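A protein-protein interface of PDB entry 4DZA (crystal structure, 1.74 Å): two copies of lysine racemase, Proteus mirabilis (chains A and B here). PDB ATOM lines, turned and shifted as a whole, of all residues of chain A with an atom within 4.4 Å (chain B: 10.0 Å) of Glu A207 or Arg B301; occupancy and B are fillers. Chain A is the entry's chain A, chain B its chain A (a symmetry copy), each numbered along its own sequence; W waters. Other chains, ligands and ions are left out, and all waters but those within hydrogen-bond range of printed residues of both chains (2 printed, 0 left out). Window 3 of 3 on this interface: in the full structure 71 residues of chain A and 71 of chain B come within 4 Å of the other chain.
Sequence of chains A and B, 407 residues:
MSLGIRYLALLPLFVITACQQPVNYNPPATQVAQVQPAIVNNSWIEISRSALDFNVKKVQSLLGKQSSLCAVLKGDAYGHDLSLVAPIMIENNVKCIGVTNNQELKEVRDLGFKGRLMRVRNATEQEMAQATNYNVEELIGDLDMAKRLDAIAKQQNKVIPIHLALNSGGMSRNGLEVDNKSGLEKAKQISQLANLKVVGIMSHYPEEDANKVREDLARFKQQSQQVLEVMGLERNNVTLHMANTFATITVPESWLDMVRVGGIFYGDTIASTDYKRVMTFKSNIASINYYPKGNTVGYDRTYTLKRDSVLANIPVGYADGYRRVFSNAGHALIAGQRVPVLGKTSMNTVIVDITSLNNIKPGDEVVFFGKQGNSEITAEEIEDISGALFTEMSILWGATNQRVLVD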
ATOM      1  N   GLY A 169       2.212 -31.167  -0.155  1.00  0.00           N
ATOM      2  CA  GLY A 169       3.123 -30.238  -0.856  1.00  0.00           C
ATOM      3  C   GLY A 169       3.646 -29.117   0.031  1.00  0.00           C
ATOM      4  O   GLY A 169       4.784 -28.693  -0.107  1.00  0.00           O
ATOM      5  N   GLY A 170       2.818 -28.667   0.973  1.00  0.00           N
ATOM      6  CA  GLY A 170       3.201 -27.641   1.934  1.00  0.00           C
ATOM      7  C   GLY A 170       2.632 -26.239   1.724  1.00  0.00           C
ATOM      8  O   GLY A 170       3.096 -25.303   2.323  1.00  0.00           O
ATOM      9  N   TYR A 205       2.011 -28.604  -5.562  1.00  0.00           N
ATOM     10  CA  TYR A 205       3.430 -28.247  -5.382  1.00  0.00           C
ATOM     11  C   TYR A 205       3.612 -26.744  -5.245  1.00  0.00           C
ATOM     12  O   TYR A 205       3.181 -25.982  -6.113  1.00  0.00           O
ATOM     13  CB  TYR A 205       4.263 -28.704  -6.599  1.00  0.00           C
ATOM     14  CG  TYR A 205       4.219 -30.193  -6.847  1.00  0.00           C
ATOM     15  CD1 TYR A 205       4.688 -31.091  -5.879  1.00  0.00           C
ATOM     16  CD2 TYR A 205       3.605 -30.713  -7.987  1.00  0.00           C
ATOM     17  CE1 TYR A 205       4.583 -32.453  -6.043  1.00  0.00           C
ATOM     18  CE2 TYR A 205       3.497 -32.106  -8.175  1.00  0.00           C
ATOM     19  CZ  TYR A 205       3.976 -32.970  -7.183  1.00  0.00           C
ATOM     20  OH  TYR A 205       3.888 -34.329  -7.355  1.00  0.00           O
ATOM     21  N   PRO A 206       4.324 -26.311  -4.192  1.00  0.00           N
ATOM     22  CA  PRO A 206       4.631 -24.928  -4.010  1.00  0.00           C
ATOM     23  C   PRO A 206       5.729 -24.376  -4.937  1.00  0.00           C
ATOM     24  O   PRO A 206       5.776 -23.190  -5.148  1.00  0.00           O
ATOM     25  CB  PRO A 206       5.093 -24.870  -2.542  1.00  0.00           C
ATOM     26  CG  PRO A 206       4.377 -25.978  -1.892  1.00  0.00           C
ATOM     27  CD  PRO A 206       4.437 -27.064  -2.937  1.00  0.00           C
ATOM     28  N   GLU A 207       6.612 -25.240  -5.458  1.00  0.00           N
ATOM     29  CA  GLU A 207       7.835 -24.754  -6.118  1.00  0.00           C
ATOM     30  C   GLU A 207       8.016 -25.486  -7.424  1.00  0.00           C
ATOM     31  O   GLU A 207       8.157 -26.710  -7.408  1.00  0.00           O
ATOM     32  CB  GLU A 207       9.065 -25.113  -5.291  1.00  0.00           C
ATOM     33  CG  GLU A 207       9.326 -24.317  -4.053  1.00  0.00           C
ATOM     34  CD  GLU A 207      10.558 -24.874  -3.299  1.00  0.00           C
ATOM     35  OE1 GLU A 207      10.489 -25.110  -2.059  1.00  0.00           O
ATOM     36  OE2 GLU A 207      11.579 -25.150  -3.983  1.00  0.00           O
ATOM     37  N   GLU A 208       8.147 -24.742  -8.515  1.00  0.00           N
ATOM     38  CA  GLU A 208       8.460 -25.307  -9.827  1.00  0.00           C
ATOM     39  C   GLU A 208       9.965 -25.673  -9.935  1.00  0.00           C
ATOM     40  O   GLU A 208      10.743 -25.005 -10.627  1.00  0.00           O
ATOM     41  CB  GLU A 208       8.069 -24.311 -10.918  1.00  0.00           C
ATOM     42  CG  GLU A 208       6.602 -23.873 -10.802  1.00  0.00           C
ATOM     43  CD  GLU A 208       6.106 -23.082 -11.994  1.00  0.00           C
ATOM     44  OE1 GLU A 208       6.905 -22.331 -12.577  1.00  0.00           O
ATOM     45  OE2 GLU A 208       4.868 -23.168 -12.312  1.00  0.00           O
ATOM     46  N   ASP A 209      10.353 -26.727  -9.220  1.00  0.00           N
ATOM     47  CA  ASP A 209      11.729 -27.232  -9.217  1.00  0.00           C
ATOM     48  C   ASP A 209      11.644 -28.752  -9.171  1.00  0.00           C
ATOM     49  O   ASP A 209      11.010 -29.327  -8.274  1.00  0.00           O
ATOM     50  CB  ASP A 209      12.465 -26.696  -7.992  1.00  0.00           C
ATOM     51  CG  ASP A 209      13.787 -27.398  -7.744  1.00  0.00           C
ATOM     52  OD1 ASP A 209      13.772 -28.593  -7.378  1.00  0.00           O
ATOM     53  OD2 ASP A 209      14.834 -26.732  -7.889  1.00  0.00           O
ATOM     54  N   LYS A 212      12.392 -30.518  -5.826  1.00  0.00           N
ATOM     55  CA  LYS A 212      11.437 -30.213  -4.763  1.00  0.00           C
ATOM     56  C   LYS A 212      10.106 -30.887  -5.073  1.00  0.00           C
ATOM     57  O   LYS A 212       9.531 -31.533  -4.201  1.00  0.00           O
ATOM     58  CB  LYS A 212      11.284 -28.712  -4.538  1.00  0.00           C
ATOM     59  CG  LYS A 212      12.433 -28.060  -3.720  1.00  0.00           C
ATOM     60  CD  LYS A 212      12.223 -28.188  -2.196  1.00  0.00           C
ATOM     61  CE  LYS A 212      13.294 -27.425  -1.384  1.00  0.00           C
ATOM     62  NZ  LYS A 212      12.738 -26.228  -0.671  1.00  0.00           N
ATOM     63  N   VAL A 213       9.712 -30.889  -6.347  1.00  0.00           N
ATOM     64  CA  VAL A 213       8.627 -31.755  -6.823  1.00  0.00           C
ATOM     65  C   VAL A 213       8.769 -33.238  -6.432  1.00  0.00           C
ATOM     66  O   VAL A 213       7.837 -33.846  -5.891  1.00  0.00           O
ATOM     67  CB  VAL A 213       8.415 -31.620  -8.360  1.00  0.00           C
ATOM     68  CG1 VAL A 213       7.520 -32.754  -8.911  1.00  0.00           C
ATOM     69  CG2 VAL A 213       7.793 -30.271  -8.710  1.00  0.00           C
ATOM     70  N   ASP A 216       8.175 -33.629  -2.548  1.00  0.00           N
ATOM     71  CA  ASP A 216       6.780 -33.441  -2.177  1.00  0.00           C
ATOM     72  C   ASP A 216       5.969 -34.605  -2.709  1.00  0.00           C
ATOM     73  O   ASP A 216       5.021 -35.049  -2.078  1.00  0.00           O
ATOM     74  CB  ASP A 216       6.234 -32.104  -2.771  1.00  0.00           C
ATOM     75  CG  ASP A 216       7.041 -30.874  -2.307  1.00  0.00           C
ATOM     76  OD1 ASP A 216       7.675 -30.916  -1.206  1.00  0.00           O
ATOM     77  OD2 ASP A 216       7.020 -29.851  -3.023  1.00  0.00           O
ATOM     78  N   GLY B 294       6.381 -23.712  11.939  1.00  0.00           N
ATOM     79  CA  GLY B 294       7.362 -24.319  11.000  1.00  0.00           C
ATOM     80  C   GLY B 294       6.813 -24.566   9.600  1.00  0.00           C
ATOM     81  O   GLY B 294       7.561 -24.676   8.637  1.00  0.00           O
ATOM     82  N   ASN B 295       5.496 -24.739   9.498  1.00  0.00           N
ATOM     83  CA  ASN B 295       4.850 -24.809   8.173  1.00  0.00           C
ATOM     84  C   ASN B 295       5.126 -23.508   7.401  1.00  0.00           C
ATOM     85  O   ASN B 295       5.338 -22.433   7.991  1.00  0.00           O
ATOM     86  CB  ASN B 295       3.321 -25.019   8.337  1.00  0.00           C
ATOM     87  CG  ASN B 295       2.906 -26.485   8.221  1.00  0.00           C
ATOM     88  OD1 ASN B 295       1.802 -26.797   7.730  1.00  0.00           O
ATOM     89  ND2 ASN B 295       3.780 -27.382   8.615  1.00  0.00           N
ATOM     90  N   THR B 296       5.045 -23.582   6.081  1.00  0.00           N
ATOM     91  CA  THR B 296       5.200 -22.383   5.271  1.00  0.00           C
ATOM     92  C   THR B 296       3.910 -22.112   4.500  1.00  0.00           C
ATOM     93  O   THR B 296       3.073 -22.972   4.413  1.00  0.00           O
ATOM     94  CB  THR B 296       6.380 -22.467   4.283  1.00  0.00           C
ATOM     95  OG1 THR B 296       6.242 -23.595   3.395  1.00  0.00           O
ATOM     96  CG2 THR B 296       7.711 -22.550   5.028  1.00  0.00           C
ATOM     97  N   VAL B 297       3.778 -20.908   3.971  1.00  0.00           N
ATOM     98  CA  VAL B 297       2.552 -20.512   3.301  1.00  0.00           C
ATOM     99  C   VAL B 297       2.772 -20.104   1.835  1.00  0.00           C
ATOM    100  O   VAL B 297       3.541 -19.176   1.516  1.00  0.00           O
ATOM    101  CB  VAL B 297       1.768 -19.416   4.067  1.00  0.00           C
ATOM    102  CG1 VAL B 297       0.385 -19.153   3.311  1.00  0.00           C
ATOM    103  CG2 VAL B 297       1.540 -19.803   5.541  1.00  0.00           C
ATOM    104  N   GLY B 298       2.057 -20.759   0.925  1.00  0.00           N
ATOM    105  CA  GLY B 298       1.910 -20.190  -0.414  1.00  0.00           C
ATOM    106  C   GLY B 298       2.999 -20.647  -1.376  1.00  0.00           C
ATOM    107  O   GLY B 298       3.914 -21.401  -0.990  1.00  0.00           O
ATOM    108  N   TYR B 299       2.922 -20.191  -2.616  1.00  0.00           N
ATOM    109  CA  TYR B 299       3.974 -20.518  -3.631  1.00  0.00           C
ATOM    110  C   TYR B 299       5.379 -20.042  -3.181  1.00  0.00           C
ATOM    111  O   TYR B 299       5.511 -18.976  -2.559  1.00  0.00           O
ATOM    112  CB  TYR B 299       3.657 -19.915  -5.016  1.00  0.00           C
ATOM    113  CG  TYR B 299       2.548 -20.631  -5.787  1.00  0.00           C
ATOM    114  CD1 TYR B 299       2.771 -21.886  -6.351  1.00  0.00           C
ATOM    115  CD2 TYR B 299       1.300 -20.017  -6.002  1.00  0.00           C
ATOM    116  CE1 TYR B 299       1.786 -22.533  -7.093  1.00  0.00           C
ATOM    117  CE2 TYR B 299       0.298 -20.672  -6.682  1.00  0.00           C
ATOM    118  CZ  TYR B 299       0.543 -21.896  -7.274  1.00  0.00           C
ATOM    119  OH  TYR B 299      -0.464 -22.550  -7.984  1.00  0.00           O
ATOM    120  N   ASP B 300       6.365 -20.883  -3.474  1.00  0.00           N
ATOM    121  CA  ASP B 300       7.794 -20.664  -3.059  1.00  0.00           C
ATOM    122  C   ASP B 300       8.001 -20.525  -1.548  1.00  0.00           C
ATOM    123  O   ASP B 300       9.039 -19.977  -1.102  1.00  0.00           O
ATOM    124  CB  ASP B 300       8.379 -19.417  -3.737  1.00  0.00           C
ATOM    125  CG  ASP B 300       8.579 -19.593  -5.236  1.00  0.00           C
ATOM    126  OD1 ASP B 300       8.591 -20.746  -5.750  1.00  0.00           O
ATOM    127  OD2 ASP B 300       8.701 -18.555  -5.911  1.00  0.00           O
ATOM    128  N   ARG B 301       7.005 -20.920  -0.757  1.00  0.00           N
ATOM    129  CA  ARG B 301       7.188 -21.027   0.708  1.00  0.00           C
ATOM    130  C   ARG B 301       7.791 -19.766   1.375  1.00  0.00           C
ATOM    131  O   ARG B 301       8.651 -19.886   2.282  1.00  0.00           O
ATOM    132  CB  ARG B 301       8.056 -22.233   1.032  1.00  0.00           C
ATOM    133  CG  ARG B 301       8.006 -23.330  -0.014  1.00  0.00           C
ATOM    134  CD  ARG B 301       8.952 -24.478   0.331  1.00  0.00           C
ATOM    135  NE  ARG B 301       8.211 -25.672   0.696  1.00  0.00           N
ATOM    136  CZ  ARG B 301       7.934 -26.668  -0.138  1.00  0.00           C
ATOM    137  NH1 ARG B 301       8.377 -26.639  -1.403  1.00  0.00           N
ATOM    138  NH2 ARG B 301       7.229 -27.704   0.295  1.00  0.00           N
ATOM    139  N   THR B 302       7.318 -18.590   0.953  1.00  0.00           N
ATOM    140  CA  THR B 302       7.917 -17.275   1.257  1.00  0.00           C
ATOM    141  C   THR B 302       7.601 -16.739   2.645  1.00  0.00           C
ATOM    142  O   THR B 302       8.161 -15.735   3.065  1.00  0.00           O
ATOM    143  CB  THR B 302       7.408 -16.210   0.236  1.00  0.00           C
ATOM    144  OG1 THR B 302       7.713 -16.636  -1.098  1.00  0.00           O
ATOM    145  CG2 THR B 302       8.075 -14.844   0.480  1.00  0.00           C
ATOM    146  N   TYR B 303       6.645 -17.349   3.316  1.00  0.00           N
ATOM    147  CA  TYR B 303       6.324 -17.017   4.704  1.00  0.00           C
ATOM    148  C   TYR B 303       6.312 -18.267   5.600  1.00  0.00           C
ATOM    149  O   TYR B 303       5.647 -19.262   5.304  1.00  0.00           O
ATOM    150  CB  TYR B 303       4.997 -16.243   4.820  1.00  0.00           C
ATOM    151  CG  TYR B 303       4.708 -15.740   6.239  1.00  0.00           C
ATOM    152  CD1 TYR B 303       5.277 -14.559   6.709  1.00  0.00           C
ATOM    153  CD2 TYR B 303       3.952 -16.512   7.148  1.00  0.00           C
ATOM    154  CE1 TYR B 303       5.031 -14.111   8.032  1.00  0.00           C
ATOM    155  CE2 TYR B 303       3.735 -16.091   8.464  1.00  0.00           C
ATOM    156  CZ  TYR B 303       4.264 -14.895   8.906  1.00  0.00           C
ATOM    157  OH  TYR B 303       3.981 -14.474  10.237  1.00  0.00           O
ATOM    158  N   THR B 304       7.108 -18.225   6.677  1.00  0.00           N
ATOM    159  CA  THR B 304       7.197 -19.341   7.632  1.00  0.00           C
ATOM    160  C   THR B 304       6.425 -19.027   8.929  1.00  0.00           C
ATOM    161  O   THR B 304       6.573 -17.931   9.507  1.00  0.00           O
ATOM    162  CB  THR B 304       8.694 -19.629   7.946  1.00  0.00           C
ATOM    163  OG1 THR B 304       9.336 -20.100   6.757  1.00  0.00           O
ATOM    164  CG2 THR B 304       8.843 -20.679   9.041  1.00  0.00           C
ATOM    165  N   LEU B 305       5.554 -19.944   9.361  1.00  0.00           N
ATOM    166  CA  LEU B 305       4.758 -19.698  10.543  1.00  0.00           C
ATOM    167  C   LEU B 305       5.689 -19.753  11.809  1.00  0.00           C
ATOM    168  O   LEU B 305       6.462 -20.688  11.967  1.00  0.00           O
ATOM    169  CB  LEU B 305       3.657 -20.744  10.660  1.00  0.00           C
ATOM    170  CG  LEU B 305       2.655 -20.753   9.488  1.00  0.00           C
ATOM    171  CD1 LEU B 305       1.655 -21.900   9.736  1.00  0.00           C
ATOM    172  CD2 LEU B 305       1.939 -19.416   9.366  1.00  0.00           C
ATOM    173  N   ARG B 324      -0.055  -9.613  -7.100  1.00  0.00           N
ATOM    174  CA  ARG B 324       1.113 -10.169  -6.427  1.00  0.00           C
ATOM    175  C   ARG B 324       1.841  -9.111  -5.629  1.00  0.00           C
ATOM    176  O   ARG B 324       2.618  -9.407  -4.712  1.00  0.00           O
ATOM    177  CB  ARG B 324       2.051 -10.728  -7.479  1.00  0.00           C
ATOM    178  CG  ARG B 324       1.673 -12.137  -7.905  1.00  0.00           C
ATOM    179  CD  ARG B 324       2.281 -13.145  -6.888  1.00  0.00           C
ATOM    180  NE  ARG B 324       1.706 -14.480  -6.866  1.00  0.00           N
ATOM    181  CZ  ARG B 324       2.268 -15.558  -7.443  1.00  0.00           C
ATOM    182  NH1 ARG B 324       3.389 -15.434  -8.145  1.00  0.00           N
ATOM    183  NH2 ARG B 324       1.701 -16.761  -7.332  1.00  0.00           N
ATOM    184  N   ASN B 328       2.667 -10.933   1.058  1.00  0.00           N
ATOM    185  CA  ASN B 328       3.360 -10.601   2.350  1.00  0.00           C
ATOM    186  C   ASN B 328       3.319  -9.115   2.676  1.00  0.00           C
ATOM    187  O   ASN B 328       4.231  -8.598   3.326  1.00  0.00           O
ATOM    188  CB  ASN B 328       4.832 -11.050   2.317  1.00  0.00           C
ATOM    189  CG  ASN B 328       4.992 -12.545   2.473  1.00  0.00           C
ATOM    190  OD1 ASN B 328       5.731 -13.180   1.706  1.00  0.00           O
ATOM    191  ND2 ASN B 328       4.271 -13.128   3.419  1.00  0.00           N
ATOM    192  N   LEU B 342      -0.573 -13.548   4.223  1.00  0.00           N
ATOM    193  CA  LEU B 342       0.615 -14.376   4.360  1.00  0.00           C
ATOM    194  C   LEU B 342       1.006 -15.001   3.032  1.00  0.00           C
ATOM    195  O   LEU B 342       0.179 -15.715   2.384  1.00  0.00           O
ATOM    196  CB  LEU B 342       0.372 -15.511   5.374  1.00  0.00           C
ATOM    197  CG  LEU B 342      -0.008 -15.098   6.801  1.00  0.00           C
ATOM    198  CD1 LEU B 342      -0.009 -16.302   7.724  1.00  0.00           C
ATOM    199  CD2 LEU B 342       0.977 -14.027   7.293  1.00  0.00           C
ATOM    200  N   GLY B 343       2.264 -14.803   2.651  1.00  0.00           N
ATOM    201  CA  GLY B 343       2.821 -15.443   1.435  1.00  0.00           C
ATOM    202  C   GLY B 343       2.345 -14.774   0.142  1.00  0.00           C
ATOM    203  O   GLY B 343       1.733 -13.725   0.163  1.00  0.00           O
ATOM    204  N   LYS B 344       2.562 -15.448  -0.962  1.00  0.00           N
ATOM    205  CA  LYS B 344       2.286 -14.887  -2.282  1.00  0.00           C
ATOM    206  C   LYS B 344       0.800 -15.044  -2.487  1.00  0.00           C
ATOM    207  O   LYS B 344       0.238 -16.083  -2.086  1.00  0.00           O
ATOM    208  CB  LYS B 344       3.048 -15.661  -3.374  1.00  0.00           C
ATOM    209  CG  LYS B 344       4.504 -15.287  -3.473  1.00  0.00           C
ATOM    210  CD  LYS B 344       5.180 -15.983  -4.632  1.00  0.00           C
ATOM    211  CE  LYS B 344       6.624 -15.528  -4.768  1.00  0.00           C
ATOM    212  NZ  LYS B 344       7.253 -16.108  -6.025  1.00  0.00           N
ATOM    213  N   THR B 345       0.178 -14.037  -3.122  1.00  0.00           N
ATOM    214  CA  THR B 345      -1.211 -14.180  -3.524  1.00  0.00           C
ATOM    215  C   THR B 345      -1.293 -15.332  -4.534  1.00  0.00           C
ATOM    216  O   THR B 345      -0.375 -15.542  -5.304  1.00  0.00           O
ATOM    217  CB  THR B 345      -1.804 -12.854  -4.070  1.00  0.00           C
ATOM    218  OG1 THR B 345      -1.090 -12.400  -5.230  1.00  0.00           O
ATOM    219  CG2 THR B 345      -1.738 -11.743  -2.999  1.00  0.00           C
HETATM  220  O   HOH W   1       3.929 -25.927   4.890  1.00  0.00           O
HETATM  221  O   HOH W   2       4.430 -23.071   1.219  1.00  0.00           O
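OD2 of Asp B300 lies within salt-bridge range of NZ of Lys B344 (2.8 Å).
The side-chain amino group (NZ) of Lys A212 is in salt-bridge range of the side-chain carboxylate (OE1) of Glu A207, at 2.9 Å.
No position is printed for both chains.
Water W1 bridges O of Gly A170 (2.8 Å) and N of Thr B296 (2.9 Å).
Water W2 lies within hydrogen-bond range of the backbone carbonyl oxygen (O) of Gly B298 (2.8 Å), the backbone carbonyl oxygen (O) of Gly A170 (2.8 Å) and the side-chain hydroxyl (OG1) of Thr B296 (2.9 Å).
Of the 18 printed residues of chain B, 5 touch a printed residue of chain A.
Hydrophobic or aromatic side chains of chain B within 4 Å of the printed part of chain A: Tyr B299.
Of the 10 printed residues of chain A, 6 touch a printed residue of chain B.
Among the printed residues, 9 pairs touch across the chains.
Of chain B, only Thr B296 (3.1 Å) comes within 4 Å of Gly A170.
Of chain B, only Arg B301 (2.7 Å) comes within 4 Å of Glu A207.
No residue of chain B comes within 4 Å of Asp A209.
Printed residues of chain B within 4 Å of Asp A216: Arg B301 (3.6 Å).
Printed residues of chain A within 4 Å of Thr B296: Gly A170.
Of the printed residues of chain A, Asp B300 touches Pro A206.
Of chain A, only Gly A169 (2.7 Å), Pro A206 (3.9 Å), Glu A207 (2.7 Å) and Asp A216 (3.6 Å) come within 4 Å of Arg B301.
The nearest residue of chain B that does not touch Glu A207 is Asp B300 (4.02 Å).
The nearest residue of chain A that does not touch Arg B301 is Lys A212 (4.2 Å).
Among the printed residues, merely in contact across the chains: Pro A206 with Tyr B299 (3.5 Å), Tyr A205 with Tyr B299 (3.8 Å), Pro A206 with Arg B301 (3.9 Å) and Pro A206 with Gly B298 (3.98 Å).
The backbone carbonyl oxygen (O) of Pro A206 is in hydrogen-bond range of the backbone NH (N) of Asp B300.
OE1 of Glu A207 is in salt-bridge range of NH1 of Arg B301, 2.7 Å away.
The backbone carbonyl oxygen (O) of Gly A169 sits at hydrogen-bond distance from the guanidinium group (NH2) of Arg B301 (2.7 Å).
The side-chain carboxylate (OD1) of Asp A216 lies within salt-bridge range of the guanidinium group (NH2) of Arg B301 (3.6 Å).
O of Thr B296 lies close to O of Gly A170, 3.1 Å away.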
